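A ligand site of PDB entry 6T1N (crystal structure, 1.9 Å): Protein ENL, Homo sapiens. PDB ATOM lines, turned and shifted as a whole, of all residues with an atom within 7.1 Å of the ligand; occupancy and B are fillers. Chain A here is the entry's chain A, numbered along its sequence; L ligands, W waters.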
ATOM      1  N   ARG A  20       8.126   6.297   6.636  1.00  0.00           N
ATOM      2  CA  ARG A  20       6.904   5.532   6.306  1.00  0.00           C
ATOM      3  C   ARG A  20       6.805   5.449   4.787  1.00  0.00           C
ATOM      4  O   ARG A  20       7.055   6.459   4.157  1.00  0.00           O
ATOM      5  CB  ARG A  20       5.702   6.284   6.894  1.00  0.00           C
ATOM      6  CG  ARG A  20       4.624   5.399   7.459  1.00  0.00           C
ATOM      7  CD  ARG A  20       3.577   6.245   8.158  1.00  0.00           C
ATOM      8  NE  ARG A  20       2.251   5.783   7.827  1.00  0.00           N
ATOM      9  CZ  ARG A  20       1.700   4.687   8.320  1.00  0.00           C
ATOM     10  NH1 ARG A  20       2.354   3.940   9.196  1.00  0.00           N
ATOM     11  NH2 ARG A  20       0.491   4.312   7.923  1.00  0.00           N
ATOM     12  N   GLU A  26      -1.028  10.763   2.569  1.00  0.00           N
ATOM     13  CA  GLU A  26      -0.949  10.530   4.031  1.00  0.00           C
ATOM     14  C   GLU A  26       0.178  11.384   4.582  1.00  0.00           C
ATOM     15  O   GLU A  26       1.287  11.314   4.043  1.00  0.00           O
ATOM     16  CB  GLU A  26      -0.753   9.052   4.332  1.00  0.00           C
ATOM     17  CG  GLU A  26      -1.019   8.713   5.776  1.00  0.00           C
ATOM     18  CD  GLU A  26      -0.078   7.673   6.311  1.00  0.00           C
ATOM     19  OE1 GLU A  26       1.150   7.778   6.025  1.00  0.00           O
ATOM     20  OE2 GLU A  26      -0.544   6.761   6.989  1.00  0.00           O
ATOM     21  N   PHE A  28       1.768  11.612   7.492  1.00  0.00           N
ATOM     22  CA  PHE A  28       2.763  11.013   8.415  1.00  0.00           C
ATOM     23  C   PHE A  28       3.952  10.490   7.603  1.00  0.00           C
ATOM     24  O   PHE A  28       3.794   9.506   6.870  1.00  0.00           O
ATOM     25  CB  PHE A  28       2.110   9.931   9.272  1.00  0.00           C
ATOM     26  CG  PHE A  28       0.827  10.356   9.933  1.00  0.00           C
ATOM     27  CD1 PHE A  28       0.796  11.436  10.791  1.00  0.00           C
ATOM     28  CD2 PHE A  28      -0.352   9.657   9.717  1.00  0.00           C
ATOM     29  CE1 PHE A  28      -0.390  11.842  11.389  1.00  0.00           C
ATOM     30  CE2 PHE A  28      -1.535  10.050  10.317  1.00  0.00           C
ATOM     31  CZ  PHE A  28      -1.551  11.137  11.161  1.00  0.00           C
ATOM     32  N   HIS A  30       6.876   9.364   9.034  1.00  0.00           N
ATOM     33  CA  HIS A  30       7.736   8.470   9.846  1.00  0.00           C
ATOM     34  C   HIS A  30       6.898   7.479  10.622  1.00  0.00           C
ATOM     35  O   HIS A  30       5.773   7.836  11.038  1.00  0.00           O
ATOM     36  CB  HIS A  30       8.630   9.264  10.789  1.00  0.00           C
ATOM     37  CG  HIS A  30       9.749   9.962  10.101  1.00  0.00           C
ATOM     38  ND1 HIS A  30       9.574  11.147   9.428  1.00  0.00           N
ATOM     39  CD2 HIS A  30      11.065   9.655  10.017  1.00  0.00           C
ATOM     40  CE1 HIS A  30      10.744  11.541   8.925  1.00  0.00           C
ATOM     41  NE2 HIS A  30      11.661  10.650   9.277  1.00  0.00           N
ATOM     42  N   TRP A  32       7.657   5.513  14.223  1.00  0.00           N
ATOM     43  CA  TRP A  32       8.603   5.492  15.362  1.00  0.00           C
ATOM     44  C   TRP A  32       8.052   4.631  16.496  1.00  0.00           C
ATOM     45  O   TRP A  32       6.847   4.296  16.498  1.00  0.00           O
ATOM     46  CB  TRP A  32       8.967   6.909  15.827  1.00  0.00           C
ATOM     47  CG  TRP A  32       7.811   7.756  16.232  1.00  0.00           C
ATOM     48  CD1 TRP A  32       7.297   8.825  15.557  1.00  0.00           C
ATOM     49  CD2 TRP A  32       7.093   7.696  17.484  1.00  0.00           C
ATOM     50  NE1 TRP A  32       6.270   9.375  16.258  1.00  0.00           N
ATOM     51  CE2 TRP A  32       6.131   8.719  17.448  1.00  0.00           C
ATOM     52  CE3 TRP A  32       7.162   6.858  18.611  1.00  0.00           C
ATOM     53  CZ2 TRP A  32       5.261   8.956  18.525  1.00  0.00           C
ATOM     54  CZ3 TRP A  32       6.282   7.063  19.646  1.00  0.00           C
ATOM     55  CH2 TRP A  32       5.360   8.115  19.613  1.00  0.00           C
ATOM     56  N   HIS A  56       2.844  14.168  22.092  1.00  0.00           N
ATOM     57  CA  HIS A  56       2.371  15.489  21.614  1.00  0.00           C
ATOM     58  C   HIS A  56       0.839  15.550  21.676  1.00  0.00           C
ATOM     59  O   HIS A  56       0.184  14.522  21.314  1.00  0.00           O
ATOM     60  CB  HIS A  56       2.895  15.767  20.228  1.00  0.00           C
ATOM     61  CG  HIS A  56       2.748  17.190  19.835  1.00  0.00           C
ATOM     62  ND1 HIS A  56       1.633  17.672  19.148  1.00  0.00           N
ATOM     63  CD2 HIS A  56       3.563  18.260  20.022  1.00  0.00           C
ATOM     64  CE1 HIS A  56       1.784  18.964  18.941  1.00  0.00           C
ATOM     65  NE2 HIS A  56       2.957  19.343  19.455  1.00  0.00           N
ATOM     66  N   ASP A  57       0.299  16.707  22.084  1.00  0.00           N
ATOM     67  CA  ASP A  57      -1.152  16.996  22.299  1.00  0.00           C
ATOM     68  C   ASP A  57      -1.968  16.661  21.029  1.00  0.00           C
ATOM     69  O   ASP A  57      -3.182  16.480  21.147  1.00  0.00           O
ATOM     70  CB  ASP A  57      -1.375  18.487  22.644  1.00  0.00           C
ATOM     71  CG  ASP A  57      -0.748  18.945  23.955  1.00  0.00           C
ATOM     72  OD1 ASP A  57      -0.116  18.120  24.614  1.00  0.00           O
ATOM     73  OD2 ASP A  57      -0.919  20.115  24.299  1.00  0.00           O
ATOM     74  N   SER A  58      -1.334  16.657  19.857  1.00  0.00           N
ATOM     75  CA  SER A  58      -1.995  16.435  18.549  1.00  0.00           C
ATOM     76  C   SER A  58      -2.356  14.958  18.358  1.00  0.00           C
ATOM     77  O   SER A  58      -3.235  14.679  17.551  1.00  0.00           O
ATOM     78  CB  SER A  58      -1.115  16.924  17.432  1.00  0.00           C
ATOM     79  OG  SER A  58       0.137  16.233  17.453  1.00  0.00           O
ATOM     80  N   PHE A  59      -1.712  14.032  19.085  1.00  0.00           N
ATOM     81  CA  PHE A  59      -2.011  12.572  18.992  1.00  0.00           C
ATOM     82  C   PHE A  59      -3.371  12.265  19.615  1.00  0.00           C
ATOM     83  O   PHE A  59      -3.767  12.871  20.603  1.00  0.00           O
ATOM     84  CB  PHE A  59      -0.917  11.748  19.668  1.00  0.00           C
ATOM     85  CG  PHE A  59       0.331  11.602  18.862  1.00  0.00           C
ATOM     86  CD1 PHE A  59       1.340  12.548  18.929  1.00  0.00           C
ATOM     87  CD2 PHE A  59       0.483  10.531  17.987  1.00  0.00           C
ATOM     88  CE1 PHE A  59       2.503  12.408  18.186  1.00  0.00           C
ATOM     89  CE2 PHE A  59       1.646  10.391  17.244  1.00  0.00           C
ATOM     90  CZ  PHE A  59       2.655  11.321  17.338  1.00  0.00           C
ATOM     91  N   PRO A  60      -4.139  11.295  19.060  1.00  0.00           N
ATOM     92  CA  PRO A  60      -5.298  10.763  19.771  1.00  0.00           C
ATOM     93  C   PRO A  60      -4.846  10.085  21.073  1.00  0.00           C
ATOM     94  O   PRO A  60      -3.795   9.461  21.054  1.00  0.00           O
ATOM     95  CB  PRO A  60      -5.930   9.782  18.765  1.00  0.00           C
ATOM     96  CG  PRO A  60      -4.753   9.376  17.858  1.00  0.00           C
ATOM     97  CD  PRO A  60      -3.872  10.616  17.789  1.00  0.00           C
ATOM     98  N   ARG A  64      -0.403   7.649  26.988  1.00  0.00           N
ATOM     99  CA  ARG A  64      -0.286   6.201  26.687  1.00  0.00           C
ATOM    100  C   ARG A  64       0.309   5.492  27.899  1.00  0.00           C
ATOM    101  O   ARG A  64       1.442   5.805  28.275  1.00  0.00           O
ATOM    102  CB  ARG A  64       0.583   6.023  25.434  1.00  0.00           C
ATOM    103  CG  ARG A  64       0.080   6.786  24.194  1.00  0.00           C
ATOM    104  CD  ARG A  64      -1.258   6.256  23.648  1.00  0.00           C
ATOM    105  NE  ARG A  64      -1.716   7.042  22.518  1.00  0.00           N
ATOM    106  CZ  ARG A  64      -1.354   6.852  21.235  1.00  0.00           C
ATOM    107  NH1 ARG A  64      -1.803   7.673  20.299  1.00  0.00           N
ATOM    108  NH2 ARG A  64      -0.533   5.890  20.902  1.00  0.00           N
ATOM    109  N   GLU A  74       4.176   2.551  19.731  1.00  0.00           N
ATOM    110  CA  GLU A  74       4.465   2.527  18.283  1.00  0.00           C
ATOM    111  C   GLU A  74       3.495   3.473  17.598  1.00  0.00           C
ATOM    112  O   GLU A  74       2.291   3.353  17.827  1.00  0.00           O
ATOM    113  CB  GLU A  74       4.351   1.107  17.741  1.00  0.00           C
ATOM    114  CG  GLU A  74       5.464   0.205  18.233  1.00  0.00           C
ATOM    115  CD  GLU A  74       5.213  -1.272  18.023  1.00  0.00           C
ATOM    116  OE1 GLU A  74       4.072  -1.753  18.333  1.00  0.00           O
ATOM    117  OE2 GLU A  74       6.136  -1.955  17.541  1.00  0.00           O
ATOM    118  N   GLU A  75       4.012   4.419  16.833  1.00  0.00           N
ATOM    119  CA  GLU A  75       3.190   5.484  16.217  1.00  0.00           C
ATOM    120  C   GLU A  75       3.729   5.830  14.831  1.00  0.00           C
ATOM    121  O   GLU A  75       4.838   5.425  14.478  1.00  0.00           O
ATOM    122  CB  GLU A  75       3.147   6.726  17.120  1.00  0.00           C
ATOM    123  CG  GLU A  75       1.924   6.791  17.978  1.00  0.00           C
ATOM    124  CD  GLU A  75       0.622   6.898  17.225  1.00  0.00           C
ATOM    125  OE1 GLU A  75       0.666   7.066  15.985  1.00  0.00           O
ATOM    126  OE2 GLU A  75      -0.453   6.823  17.882  1.00  0.00           O
ATOM    127  N   SER A  76       2.928   6.572  14.086  1.00  0.00           N
ATOM    128  CA  SER A  76       3.356   7.353  12.911  1.00  0.00           C
ATOM    129  C   SER A  76       3.288   8.829  13.274  1.00  0.00           C
ATOM    130  O   SER A  76       2.592   9.159  14.266  1.00  0.00           O
ATOM    131  CB  SER A  76       2.506   7.015  11.730  1.00  0.00           C
ATOM    132  OG  SER A  76       1.140   7.176  12.065  1.00  0.00           O
ATOM    133  N   GLY A  77       4.082   9.667  12.604  1.00  0.00           N
ATOM    134  CA  GLY A  77       4.138  11.119  12.889  1.00  0.00           C
ATOM    135  C   GLY A  77       4.839  11.882  11.795  1.00  0.00           C
ATOM    136  O   GLY A  77       5.428  11.247  10.900  1.00  0.00           O
ATOM    137  N   TYR A  78       4.840  13.194  11.873  1.00  0.00           N
ATOM    138  CA  TYR A  78       5.475  14.083  10.874  1.00  0.00           C
ATOM    139  C   TYR A  78       6.559  14.964  11.522  1.00  0.00           C
ATOM    140  O   TYR A  78       7.151  15.783  10.783  1.00  0.00           O
ATOM    141  CB  TYR A  78       4.426  14.933  10.147  1.00  0.00           C
ATOM    142  CG  TYR A  78       3.361  15.553  11.009  1.00  0.00           C
ATOM    143  CD1 TYR A  78       3.614  16.712  11.729  1.00  0.00           C
ATOM    144  CD2 TYR A  78       2.083  15.024  11.054  1.00  0.00           C
ATOM    145  CE1 TYR A  78       2.625  17.311  12.497  1.00  0.00           C
ATOM    146  CE2 TYR A  78       1.078  15.624  11.805  1.00  0.00           C
ATOM    147  CZ  TYR A  78       1.359  16.760  12.537  1.00  0.00           C
ATOM    148  OH  TYR A  78       0.370  17.345  13.270  1.00  0.00           O
ATOM    149  N   ALA A  79       6.841  14.798  12.820  1.00  0.00           N
ATOM    150  CA  ALA A  79       7.862  15.596  13.540  1.00  0.00           C
ATOM    151  C   ALA A  79       8.252  14.939  14.855  1.00  0.00           C
ATOM    152  O   ALA A  79       7.398  14.290  15.494  1.00  0.00           O
ATOM    153  CB  ALA A  79       7.361  17.022  13.767  1.00  0.00           C
ATOM    154  N   GLY A  80       9.514  15.158  15.269  1.00  0.00           N
ATOM    155  CA  GLY A  80      10.005  14.861  16.613  1.00  0.00           C
ATOM    156  C   GLY A  80       9.405  15.789  17.626  1.00  0.00           C
ATOM    157  O   GLY A  80       8.799  16.765  17.217  1.00  0.00           O
ATOM    158  N   PHE A  81       9.515  15.448  18.893  1.00  0.00           N
ATOM    159  CA  PHE A  81       9.034  16.270  20.041  1.00  0.00           C
ATOM    160  C   PHE A  81       9.702  15.754  21.310  1.00  0.00           C
ATOM    161  O   PHE A  81      10.339  14.668  21.273  1.00  0.00           O
ATOM    162  CB  PHE A  81       7.506  16.215  20.178  1.00  0.00           C
ATOM    163  CG  PHE A  81       6.924  14.825  20.269  1.00  0.00           C
ATOM    164  CD1 PHE A  81       6.634  14.101  19.128  1.00  0.00           C
ATOM    165  CD2 PHE A  81       6.588  14.270  21.501  1.00  0.00           C
ATOM    166  CE1 PHE A  81       6.073  12.825  19.222  1.00  0.00           C
ATOM    167  CE2 PHE A  81       6.055  13.005  21.590  1.00  0.00           C
ATOM    168  CZ  PHE A  81       5.776  12.290  20.452  1.00  0.00           C
ATOM    169  N   ILE A  82       9.521  16.509  22.383  1.00  0.00           N
ATOM    170  CA  ILE A  82       9.952  16.155  23.752  1.00  0.00           C
ATOM    171  C   ILE A  82       8.842  15.379  24.412  1.00  0.00           C
ATOM    172  O   ILE A  82       7.683  15.926  24.500  1.00  0.00           O
ATOM    173  CB  ILE A  82      10.328  17.417  24.552  1.00  0.00           C
ATOM    174  CG1 ILE A  82      11.406  18.228  23.839  1.00  0.00           C
ATOM    175  CG2 ILE A  82      10.734  17.039  25.965  1.00  0.00           C
ATOM    176  CD1 ILE A  82      12.593  17.403  23.373  1.00  0.00           C
ATOM    177  N   LEU A 104      12.492  12.556  21.475  1.00  0.00           N
ATOM    178  CA  LEU A 104      12.035  11.755  20.314  1.00  0.00           C
ATOM    179  C   LEU A 104      12.259  12.547  19.040  1.00  0.00           C
ATOM    180  O   LEU A 104      11.331  13.218  18.589  1.00  0.00           O
ATOM    181  CB  LEU A 104      10.561  11.388  20.454  1.00  0.00           C
ATOM    182  CG  LEU A 104      10.084  10.369  19.425  1.00  0.00           C
ATOM    183  CD1 LEU A 104      10.161   8.963  19.995  1.00  0.00           C
ATOM    184  CD2 LEU A 104       8.686  10.671  18.949  1.00  0.00           C
ATOM    185  N   LEU A 106      13.315  12.392  14.818  1.00  0.00           N
ATOM    186  CA  LEU A 106      13.190  11.522  13.618  1.00  0.00           C
ATOM    187  C   LEU A 106      14.437  11.668  12.736  1.00  0.00           C
ATOM    188  O   LEU A 106      15.168  12.670  12.875  1.00  0.00           O
ATOM    189  CB  LEU A 106      11.924  11.937  12.873  1.00  0.00           C
ATOM    190  CG  LEU A 106      10.661  12.037  13.718  1.00  0.00           C
ATOM    191  CD1 LEU A 106       9.466  12.379  12.848  1.00  0.00           C
ATOM    192  CD2 LEU A 106      10.398  10.752  14.477  1.00  0.00           C
HETATM  193  C1  LIG L   1       3.419  18.064  16.189  1.00  0.00           C
HETATM  194  C2  LIG L   1       2.725  16.947  15.748  1.00  0.00           C
HETATM  195  N1  LIG L   1      -1.892   6.984  14.748  1.00  0.00           N
HETATM  196  C3  LIG L   1       3.320  15.680  15.786  1.00  0.00           C
HETATM  197  C4  LIG L   1       4.606  15.557  16.297  1.00  0.00           C
HETATM  198  C5  LIG L   1       5.303  16.668  16.746  1.00  0.00           C
HETATM  199  C6  LIG L   1       2.608  14.487  15.203  1.00  0.00           C
HETATM  200  C7  LIG L   1       0.367  13.378  15.110  1.00  0.00           C
HETATM  201  C8  LIG L   1      -1.006  13.630  15.294  1.00  0.00           C
HETATM  202  C9  LIG L   1      -1.948  12.622  15.123  1.00  0.00           C
HETATM  203  C10 LIG L   1      -1.503  11.361  14.749  1.00  0.00           C
HETATM  204  C11 LIG L   1      -1.233   9.269  14.110  1.00  0.00           C
HETATM  205  C12 LIG L   1      -1.604   7.893  13.637  1.00  0.00           C
HETATM  206  C13 LIG L   1      -3.249   7.217  15.290  1.00  0.00           C
HETATM  207  C14 LIG L   1      -3.566   6.303  16.472  1.00  0.00           C
HETATM  208  C15 LIG L   1      -3.390   4.841  16.088  1.00  0.00           C
HETATM  209  C16 LIG L   1      -2.031   4.612  15.460  1.00  0.00           C
HETATM  210  C17 LIG L   1      -1.794   5.585  14.310  1.00  0.00           C
HETATM  211  C18 LIG L   1      -0.155  11.087  14.547  1.00  0.00           C
HETATM  212  C19 LIG L   1       0.801  12.099  14.728  1.00  0.00           C
HETATM  213  O1  LIG L   1       3.239  13.648  14.562  1.00  0.00           O
HETATM  214  C20 LIG L   1       4.702  17.915  16.685  1.00  0.00           C
HETATM  215 CL1  LIG L   1       5.581  19.326  17.228  1.00  0.00          CL
HETATM  216  N2  LIG L   1       1.262  14.441  15.411  1.00  0.00           N
HETATM  217  N3  LIG L   1      -0.005   9.750  14.154  1.00  0.00           N
HETATM  218  N4  LIG L   1      -2.171  10.185  14.460  1.00  0.00           N
HETATM  219  O   HOH W   1       5.595  12.150  15.579  1.00  0.00           O
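The backbone carbonyl oxygen (O) of Ser 76 is in hydrogen-bond range of a nitrogen (N3) of the ligand. A nitrogen (N1) of the ligand lies within salt-bridge range of the side-chain carboxylate (OE1) of Glu 75 (2.8 Å). N of Tyr 78 sits at hydrogen-bond distance from O1 of the ligand (3.2 Å). The side-chain hydroxyl (OG) of Ser 58 lies within hydrogen-bond range of a nitrogen (N2) of the ligand, at 2.9 Å.
The backbone carbonyl oxygen (O) of Glu 75 sits at hydrogen-bond distance from the backbone NH (N) of Trp 32 (2.8 Å). The backbone carbonyl oxygen of His 30 lies within hydrogen-bond range of the backbone NH of Gly 77, 2.9 Å away. OG of Ser 58 lies within hydrogen-bond range of ND1 of His 56 (2.7 Å). The backbone carbonyl oxygen (O) of Pro 60 sits at hydrogen-bond distance from the guanidinium group (NH1) of Arg 64. OE2 of Glu 75 is in salt-bridge range of NH1 of Arg 64 (2.9 Å). N of Phe 81 is in hydrogen-bond range of O of Leu 104 (2.9 Å).
Phe 28 touches the ligand. His 56 touches the ligand (CE1 to C1, 3.3 Å). Phe 59 touches the ligand (CE2 to C19, 3.2 Å). Pro 60 touches the ligand (CG to C14, 3.6 Å). CA of Gly 77 touches O1 of the ligand (3.2 Å). O of Ala 79 touches C4 of the ligand (3.2 Å). Gly 80 touches the ligand (O to C5, 3.5 Å). CD1 of Phe 81 touches C5 of the ligand, 3.7 Å away. Hydrophobic or aromatic side chains that line the ligand: Phe 28, His 56, Phe 59, Pro 60, Tyr 78, Ala 79 and Phe 81. Within 4 Å of the ligand: Phe 28, His 56, Ser 58, Phe 59, Pro 60, Glu 75, Ser 76, Gly 77, Tyr 78, Ala 79, Gly 80 and Phe 81. The nearest printed residue that does not touch the ligand is Arg 64 (4.4 Å).
Water W1 lies within hydrogen-bond range of the backbone carbonyl oxygen of Ala 79, the indole nitrogen of Trp 32 and an oxygen (O1) of the ligand.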
